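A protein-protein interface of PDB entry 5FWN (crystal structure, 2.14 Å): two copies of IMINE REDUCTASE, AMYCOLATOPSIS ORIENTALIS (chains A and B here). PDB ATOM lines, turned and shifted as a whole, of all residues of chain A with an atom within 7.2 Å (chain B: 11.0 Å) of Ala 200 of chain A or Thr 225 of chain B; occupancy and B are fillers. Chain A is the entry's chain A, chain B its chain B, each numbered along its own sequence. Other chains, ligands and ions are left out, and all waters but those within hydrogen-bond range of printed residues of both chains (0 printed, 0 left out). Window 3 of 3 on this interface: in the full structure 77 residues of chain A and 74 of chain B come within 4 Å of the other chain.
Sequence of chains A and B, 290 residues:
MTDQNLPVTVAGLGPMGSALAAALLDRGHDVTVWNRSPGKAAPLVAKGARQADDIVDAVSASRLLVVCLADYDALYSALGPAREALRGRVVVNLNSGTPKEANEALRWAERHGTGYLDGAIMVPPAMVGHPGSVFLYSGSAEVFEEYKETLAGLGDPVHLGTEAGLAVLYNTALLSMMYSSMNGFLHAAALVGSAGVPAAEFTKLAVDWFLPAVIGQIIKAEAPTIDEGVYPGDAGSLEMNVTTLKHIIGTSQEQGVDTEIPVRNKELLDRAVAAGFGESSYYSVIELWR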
ATOM      1  N   VAL A 197       8.559  10.290  17.551  1.00  0.00           N
ATOM      2  CA  VAL A 197       9.633  11.297  17.408  1.00  0.00           C
ATOM      3  C   VAL A 197      10.223  11.588  18.796  1.00  0.00           C
ATOM      4  O   VAL A 197       9.475  11.739  19.745  1.00  0.00           O
ATOM      5  CB  VAL A 197       9.105  12.618  16.790  1.00  0.00           C
ATOM      6  CG1 VAL A 197      10.192  13.674  16.686  1.00  0.00           C
ATOM      7  CG2 VAL A 197       8.522  12.362  15.418  1.00  0.00           C
ATOM      8  N   PRO A 198      11.550  11.611  18.928  1.00  0.00           N
ATOM      9  CA  PRO A 198      12.130  11.880  20.242  1.00  0.00           C
ATOM     10  C   PRO A 198      11.911  13.351  20.662  1.00  0.00           C
ATOM     11  O   PRO A 198      12.010  14.242  19.838  1.00  0.00           O
ATOM     12  CB  PRO A 198      13.598  11.545  20.062  1.00  0.00           C
ATOM     13  CG  PRO A 198      13.862  11.596  18.598  1.00  0.00           C
ATOM     14  CD  PRO A 198      12.559  11.289  17.909  1.00  0.00           C
ATOM     15  N   ALA A 199      11.597  13.564  21.927  1.00  0.00           N
ATOM     16  CA  ALA A 199      11.221  14.886  22.400  1.00  0.00           C
ATOM     17  C   ALA A 199      12.372  15.883  22.457  1.00  0.00           C
ATOM     18  O   ALA A 199      12.167  17.042  22.151  1.00  0.00           O
ATOM     19  CB  ALA A 199      10.552  14.785  23.753  1.00  0.00           C
ATOM     20  N   ALA A 200      13.585  15.418  22.756  1.00  0.00           N
ATOM     21  CA  ALA A 200      14.731  16.287  22.908  1.00  0.00           C
ATOM     22  C   ALA A 200      14.945  17.094  21.643  1.00  0.00           C
ATOM     23  O   ALA A 200      15.015  18.340  21.708  1.00  0.00           O
ATOM     24  CB  ALA A 200      16.006  15.504  23.218  1.00  0.00           C
ATOM     25  N   GLU A 201      15.053  16.384  20.506  1.00  0.00           N
ATOM     26  CA  GLU A 201      15.385  17.009  19.206  1.00  0.00           C
ATOM     27  C   GLU A 201      14.260  17.910  18.706  1.00  0.00           C
ATOM     28  O   GLU A 201      14.494  18.997  18.166  1.00  0.00           O
ATOM     29  CB  GLU A 201      15.683  15.942  18.139  1.00  0.00           C
ATOM     30  N   PHE A 202      13.021  17.464  18.878  1.00  0.00           N
ATOM     31  CA  PHE A 202      11.930  18.317  18.545  1.00  0.00           C
ATOM     32  C   PHE A 202      11.946  19.582  19.419  1.00  0.00           C
ATOM     33  O   PHE A 202      11.659  20.675  18.952  1.00  0.00           O
ATOM     34  CB  PHE A 202      10.622  17.615  18.765  1.00  0.00           C
ATOM     35  CG  PHE A 202       9.447  18.494  18.509  1.00  0.00           C
ATOM     36  CD1 PHE A 202       9.108  18.850  17.195  1.00  0.00           C
ATOM     37  CD2 PHE A 202       8.665  18.964  19.551  1.00  0.00           C
ATOM     38  CE1 PHE A 202       8.011  19.656  16.942  1.00  0.00           C
ATOM     39  CE2 PHE A 202       7.591  19.815  19.289  1.00  0.00           C
ATOM     40  CZ  PHE A 202       7.259  20.137  17.990  1.00  0.00           C
ATOM     41  N   THR A 203      12.227  19.404  20.704  1.00  0.00           N
ATOM     42  CA  THR A 203      12.215  20.541  21.648  1.00  0.00           C
ATOM     43  C   THR A 203      13.193  21.631  21.233  1.00  0.00           C
ATOM     44  O   THR A 203      12.833  22.834  21.214  1.00  0.00           O
ATOM     45  CB  THR A 203      12.430  20.072  23.113  1.00  0.00           C
ATOM     46  OG1 THR A 203      11.342  19.183  23.463  1.00  0.00           O
ATOM     47  CG2 THR A 203      12.387  21.259  24.039  1.00  0.00           C
ATOM     48  N   LYS A 204      14.406  21.199  20.875  1.00  0.00           N
ATOM     49  CA  LYS A 204      15.434  22.074  20.391  1.00  0.00           C
ATOM     50  C   LYS A 204      14.985  22.764  19.118  1.00  0.00           C
ATOM     51  O   LYS A 204      15.198  23.969  18.975  1.00  0.00           O
ATOM     52  CB  LYS A 204      16.781  21.314  20.179  1.00  0.00           C
ATOM     53  CG  LYS A 204      17.503  20.940  21.515  1.00  0.00           C
ATOM     54  CD  LYS A 204      18.802  20.120  21.390  1.00  0.00           C
ATOM     55  N   LEU A 205      14.373  22.041  18.179  1.00  0.00           N
ATOM     56  CA  LEU A 205      13.903  22.695  16.954  1.00  0.00           C
ATOM     57  C   LEU A 205      12.847  23.763  17.293  1.00  0.00           C
ATOM     58  O   LEU A 205      12.870  24.884  16.756  1.00  0.00           O
ATOM     59  CB  LEU A 205      13.356  21.697  15.957  1.00  0.00           C
ATOM     60  CG  LEU A 205      12.746  22.240  14.651  1.00  0.00           C
ATOM     61  CD1 LEU A 205      13.819  22.731  13.680  1.00  0.00           C
ATOM     62  CD2 LEU A 205      11.873  21.192  13.977  1.00  0.00           C
ATOM     63  N   ALA A 206      11.916  23.394  18.162  1.00  0.00           N
ATOM     64  CA  ALA A 206      10.780  24.263  18.516  1.00  0.00           C
ATOM     65  C   ALA A 206      11.234  25.503  19.261  1.00  0.00           C
ATOM     66  O   ALA A 206      10.729  26.593  18.984  1.00  0.00           O
ATOM     67  CB  ALA A 206       9.758  23.518  19.371  1.00  0.00           C
ATOM     68  N   TYR B 170       5.417  17.541  11.914  1.00  0.00           N
ATOM     69  CA  TYR B 170       6.163  18.630  12.537  1.00  0.00           C
ATOM     70  C   TYR B 170       5.478  19.992  12.315  1.00  0.00           C
ATOM     71  O   TYR B 170       5.377  20.786  13.244  1.00  0.00           O
ATOM     72  CB  TYR B 170       7.597  18.729  12.002  1.00  0.00           C
ATOM     73  CG  TYR B 170       8.621  17.844  12.671  1.00  0.00           C
ATOM     74  CD1 TYR B 170       8.625  16.492  12.436  1.00  0.00           C
ATOM     75  CD2 TYR B 170       9.647  18.362  13.442  1.00  0.00           C
ATOM     76  CE1 TYR B 170       9.574  15.664  13.005  1.00  0.00           C
ATOM     77  CE2 TYR B 170      10.602  17.546  14.009  1.00  0.00           C
ATOM     78  CZ  TYR B 170      10.550  16.197  13.778  1.00  0.00           C
ATOM     79  OH  TYR B 170      11.484  15.355  14.250  1.00  0.00           O
ATOM     80  N   LEU B 174       4.139  22.343  15.272  1.00  0.00           N
ATOM     81  CA  LEU B 174       4.701  23.645  15.488  1.00  0.00           C
ATOM     82  C   LEU B 174       3.617  24.695  15.366  1.00  0.00           C
ATOM     83  O   LEU B 174       3.544  25.597  16.183  1.00  0.00           O
ATOM     84  CB  LEU B 174       5.845  23.927  14.521  1.00  0.00           C
ATOM     85  CG  LEU B 174       7.081  23.058  14.803  1.00  0.00           C
ATOM     86  CD1 LEU B 174       8.031  23.197  13.624  1.00  0.00           C
ATOM     87  CD2 LEU B 174       7.793  23.393  16.100  1.00  0.00           C
ATOM     88  N   GLY B 216      11.319  29.989  26.301  1.00  0.00           N
ATOM     89  CA  GLY B 216      12.161  28.957  25.689  1.00  0.00           C
ATOM     90  C   GLY B 216      12.946  28.148  26.703  1.00  0.00           C
ATOM     91  O   GLY B 216      12.980  26.882  26.681  1.00  0.00           O
ATOM     92  N   ILE B 218      12.436  27.859  30.043  1.00  0.00           N
ATOM     93  CA  ILE B 218      11.556  27.052  30.867  1.00  0.00           C
ATOM     94  C   ILE B 218      11.040  25.790  30.171  1.00  0.00           C
ATOM     95  O   ILE B 218      10.956  24.738  30.798  1.00  0.00           O
ATOM     96  CB  ILE B 218      10.399  27.889  31.443  1.00  0.00           C
ATOM     97  CG1 ILE B 218      10.983  28.693  32.583  1.00  0.00           C
ATOM     98  CG2 ILE B 218       9.320  27.019  32.044  1.00  0.00           C
ATOM     99  CD1 ILE B 218      10.106  29.810  32.995  1.00  0.00           C
ATOM    100  N   ILE B 219      10.641  25.908  28.905  1.00  0.00           N
ATOM    101  CA  ILE B 219      10.258  24.728  28.118  1.00  0.00           C
ATOM    102  C   ILE B 219      11.371  23.658  28.145  1.00  0.00           C
ATOM    103  O   ILE B 219      11.122  22.510  28.522  1.00  0.00           O
ATOM    104  CB  ILE B 219       9.851  25.084  26.679  1.00  0.00           C
ATOM    105  CG1 ILE B 219       8.464  25.736  26.693  1.00  0.00           C
ATOM    106  CG2 ILE B 219       9.852  23.848  25.786  1.00  0.00           C
ATOM    107  CD1 ILE B 219       8.100  26.431  25.417  1.00  0.00           C
ATOM    108  N   LYS B 220      12.591  24.057  27.816  1.00  0.00           N
ATOM    109  CA  LYS B 220      13.718  23.122  27.846  1.00  0.00           C
ATOM    110  C   LYS B 220      13.978  22.547  29.233  1.00  0.00           C
ATOM    111  O   LYS B 220      14.350  21.384  29.362  1.00  0.00           O
ATOM    112  CB  LYS B 220      14.987  23.783  27.391  1.00  0.00           C
ATOM    113  CG  LYS B 220      15.057  24.027  25.908  1.00  0.00           C
ATOM    114  CD  LYS B 220      16.386  24.725  25.663  1.00  0.00           C
ATOM    115  CE  LYS B 220      16.766  24.784  24.226  1.00  0.00           C
ATOM    116  NZ  LYS B 220      17.836  25.826  24.079  1.00  0.00           N
ATOM    117  N   ALA B 221      13.785  23.367  30.257  1.00  0.00           N
ATOM    118  CA  ALA B 221      13.994  22.930  31.629  1.00  0.00           C
ATOM    119  C   ALA B 221      12.906  21.914  32.015  1.00  0.00           C
ATOM    120  O   ALA B 221      13.172  21.003  32.735  1.00  0.00           O
ATOM    121  CB  ALA B 221      13.977  24.129  32.567  1.00  0.00           C
ATOM    122  N   GLU B 222      11.704  21.915  31.913  1.00  0.00           N
ATOM    123  CA  GLU B 222      10.587  20.997  31.912  1.00  0.00           C
ATOM    124  C   GLU B 222      10.786  19.855  30.937  1.00  0.00           C
ATOM    125  O   GLU B 222      10.228  18.786  31.156  1.00  0.00           O
ATOM    126  CB  GLU B 222       9.293  21.743  31.582  1.00  0.00           C
ATOM    127  CG  GLU B 222       8.883  22.770  32.626  1.00  0.00           C
ATOM    128  CD  GLU B 222       8.701  22.157  34.003  1.00  0.00           C
ATOM    129  OE1 GLU B 222       8.153  21.039  34.089  1.00  0.00           O
ATOM    130  OE2 GLU B 222       9.103  22.796  34.997  1.00  0.00           O
ATOM    131  N   ALA B 223      11.430  19.937  29.847  1.00  0.00           N
ATOM    132  CA  ALA B 223      11.542  18.749  28.951  1.00  0.00           C
ATOM    133  C   ALA B 223      12.397  17.724  29.684  1.00  0.00           C
ATOM    134  O   ALA B 223      13.543  18.007  29.982  1.00  0.00           O
ATOM    135  CB  ALA B 223      12.164  19.136  27.644  1.00  0.00           C
ATOM    136  N   PRO B 224      11.817  16.559  30.071  1.00  0.00           N
ATOM    137  CA  PRO B 224      12.642  15.634  30.897  1.00  0.00           C
ATOM    138  C   PRO B 224      13.864  15.045  30.175  1.00  0.00           C
ATOM    139  O   PRO B 224      14.749  14.483  30.844  1.00  0.00           O
ATOM    140  CB  PRO B 224      11.662  14.533  31.345  1.00  0.00           C
ATOM    141  CG  PRO B 224      10.420  14.712  30.543  1.00  0.00           C
ATOM    142  CD  PRO B 224      10.419  16.081  29.912  1.00  0.00           C
ATOM    143  N   THR B 225      13.932  15.182  28.858  1.00  0.00           N
ATOM    144  CA  THR B 225      15.071  14.651  28.124  1.00  0.00           C
ATOM    145  C   THR B 225      16.164  15.684  27.812  1.00  0.00           C
ATOM    146  O   THR B 225      17.103  15.357  27.128  1.00  0.00           O
ATOM    147  CB  THR B 225      14.592  13.962  26.804  1.00  0.00           C
ATOM    148  OG1 THR B 225      13.764  14.858  26.052  1.00  0.00           O
ATOM    149  CG2 THR B 225      13.805  12.718  27.120  1.00  0.00           C
ATOM    150  N   ILE B 226      16.044  16.917  28.281  1.00  0.00           N
ATOM    151  CA  ILE B 226      17.055  17.948  27.998  1.00  0.00           C
ATOM    152  C   ILE B 226      17.875  18.214  29.270  1.00  0.00           C
ATOM    153  O   ILE B 226      17.312  18.360  30.352  1.00  0.00           O
ATOM    154  CB  ILE B 226      16.377  19.238  27.453  1.00  0.00           C
ATOM    155  CG1 ILE B 226      15.822  19.027  26.023  1.00  0.00           C
ATOM    156  CG2 ILE B 226      17.334  20.424  27.510  1.00  0.00           C
ATOM    157  CD1 ILE B 226      16.881  19.029  24.935  1.00  0.00           C
ATOM    158  N   SER B 281       5.223  17.790  38.162  1.00  0.00           N
ATOM    159  CA  SER B 281       5.882  18.759  37.320  1.00  0.00           C
ATOM    160  C   SER B 281       4.895  19.457  36.376  1.00  0.00           C
ATOM    161  O   SER B 281       3.855  18.901  36.042  1.00  0.00           O
ATOM    162  CB  SER B 281       6.914  18.032  36.501  1.00  0.00           C
ATOM    163  OG  SER B 281       6.206  17.211  35.572  1.00  0.00           O
ATOM    164  N   TYR B 283       5.428  19.682  33.187  1.00  0.00           N
ATOM    165  CA  TYR B 283       5.450  18.910  32.007  1.00  0.00           C
ATOM    166  C   TYR B 283       4.376  17.797  32.016  1.00  0.00           C
ATOM    167  O   TYR B 283       3.817  17.493  30.940  1.00  0.00           O
ATOM    168  CB  TYR B 283       6.824  18.324  31.788  1.00  0.00           C
ATOM    169  CG  TYR B 283       7.038  17.938  30.365  1.00  0.00           C
ATOM    170  CD1 TYR B 283       7.524  18.873  29.448  1.00  0.00           C
ATOM    171  CD2 TYR B 283       6.752  16.657  29.921  1.00  0.00           C
ATOM    172  CE1 TYR B 283       7.745  18.527  28.136  1.00  0.00           C
ATOM    173  CE2 TYR B 283       6.956  16.294  28.598  1.00  0.00           C
ATOM    174  CZ  TYR B 283       7.437  17.242  27.714  1.00  0.00           C
ATOM    175  OH  TYR B 283       7.657  16.912  26.409  1.00  0.00           O
ATOM    176  N   SER B 284       4.062  17.240  33.196  1.00  0.00           N
ATOM    177  CA  SER B 284       3.053  16.157  33.334  1.00  0.00           C
ATOM    178  C   SER B 284       1.659  16.532  32.813  1.00  0.00           C
ATOM    179  O   SER B 284       0.878  15.650  32.463  1.00  0.00           O
ATOM    180  CB  SER B 284       2.962  15.646  34.797  1.00  0.00           C
ATOM    181  OG  SER B 284       2.333  16.631  35.619  1.00  0.00           O
ATOM    182  N   ILE B 286       1.107  17.166  29.924  1.00  0.00           N
ATOM    183  CA  ILE B 286       1.048  16.492  28.605  1.00  0.00           C
ATOM    184  C   ILE B 286       0.361  15.113  28.675  1.00  0.00           C
ATOM    185  O   ILE B 286      -0.296  14.689  27.693  1.00  0.00           O
ATOM    186  CB  ILE B 286       2.457  16.305  28.055  1.00  0.00           C
ATOM    187  CG1 ILE B 286       2.422  16.079  26.562  1.00  0.00           C
ATOM    188  CG2 ILE B 286       3.227  15.181  28.830  1.00  0.00           C
ATOM    189  CD1 ILE B 286       3.830  15.965  25.945  1.00  0.00           C
ATOM    190  N   GLU B 287       0.463  14.476  29.849  1.00  0.00           N
ATOM    191  CA  GLU B 287      -0.199  13.209  30.097  1.00  0.00           C
ATOM    192  C   GLU B 287      -1.716  13.312  30.048  1.00  0.00           C
ATOM    193  O   GLU B 287      -2.353  12.322  29.839  1.00  0.00           O
ATOM    194  CB  GLU B 287       0.251  12.551  31.422  1.00  0.00           C
ATOM    195  CG  GLU B 287       1.755  12.290  31.571  1.00  0.00           C
ATOM    196  CD  GLU B 287       2.380  11.589  30.361  1.00  0.00           C
ATOM    197  OE1 GLU B 287       1.674  10.903  29.578  1.00  0.00           O
ATOM    198  OE2 GLU B 287       3.555  11.753  30.125  1.00  0.00           O
ATOM    199  N   ARG B 290      -2.577  12.136  25.941  1.00  0.00           N
ATOM    200  CA  ARG B 290      -2.140  10.923  25.267  1.00  0.00           C
ATOM    201  C   ARG B 290      -2.277   9.710  26.162  1.00  0.00           C
ATOM    202  O   ARG B 290      -2.598   9.881  27.354  1.00  0.00           O
ATOM    203  CB  ARG B 290      -0.696  11.129  24.888  1.00  0.00           C
ATOM    204  CG  ARG B 290       0.241  11.358  26.052  1.00  0.00           C
ATOM    205  CD  ARG B 290       1.634  11.541  25.506  1.00  0.00           C
ATOM    206  NE  ARG B 290       2.634  11.770  26.511  1.00  0.00           N
ATOM    207  CZ  ARG B 290       3.897  12.127  26.240  1.00  0.00           C
ATOM    208  NH1 ARG B 290       4.328  12.295  24.980  1.00  0.00           N
ATOM    209  NH2 ARG B 290       4.732  12.344  27.232  1.00  0.00           N
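No position is printed for both chains.
Among the printed residues, merely in contact across the chains: Val 197 of chain A with Tyr 170 of chain B (3.2 Å), Ala 199 of chain A with Thr 225 of chain B (3.95 Å), Ala 200 of chain A with Ile 226 of chain B (3.8 Å), Phe 202 of chain A with Tyr 170 of chain B (3.8 Å), Phe 202 of chain A with Leu 174 of chain B (3.8 Å), Lys 204 of chain A with Ile 226 of chain B (3.97 Å), Leu 205 of chain A with Tyr 170 of chain B (3.6 Å) and Ala 206 of chain A with Leu 174 of chain B (3.8 Å).
Ala 200 of chain A touches two residues of chain B. Of chain A, only Ala 199 and Ala 200 come within 4 Å of Thr 225 of chain B. No residue of chain B comes within 4 Å of Pro 198 of chain A. Of chain B, only Thr 225 comes within 4 Å of Ala 199 of chain A. No residue of chain B comes within 4 Å of Glu 201 of chain A. No residue of chain B comes within 4 Å of Thr 203 of chain A. Lys 204 of chain A touches just one residue of chain B: Ile 226 (3.97 Å). Printed residues of chain A within 4 Å of Ile 226 of chain B: Ala 200 (3.8 Å) and Lys 204 (3.97 Å). Printed residues of chain B within 4 Å of Ala 206 of chain A: Leu 174. Of the printed residues of chain B, Phe 202 of chain A touches Tyr 170 (3.8 Å) and Leu 174 (3.8 Å). The nearest residue of chain B that does not touch Ala 200 of chain A is Ala 223 of chain B (6.1 Å). The nearest residue of chain A that does not touch Thr 225 of chain B is Thr 203 of chain A (5.6 Å).
The backbone carbonyl oxygen (O) of Ala 199 of chain A is in hydrogen-bond range of the side-chain hydroxyl (OG1) of Thr 203 of chain A (2.6 Å).
The backbone NH (N) of Ala 200 of chain A is in hydrogen-bond range of the side-chain hydroxyl (OG1) of Thr 225 of chain B.
Of the 10 printed residues of chain A, 7 touch a printed residue of chain B. Hydrophobic or aromatic side chains of chain A that line the printed part of chain B: Val 197, Ala 199, Ala 200, Phe 202, Leu 205 and Ala 206. Of the 18 printed residues of chain B, 4 touch a printed residue of chain A. Hydrophobic or aromatic side chains of chain B that line the printed part of chain A: Tyr 170, Leu 174 and Ile 226. Among the printed residues, no Asp or Glu carboxylate lies within 4 Å of a Lys or Arg side-chain nitrogen of the other chain.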
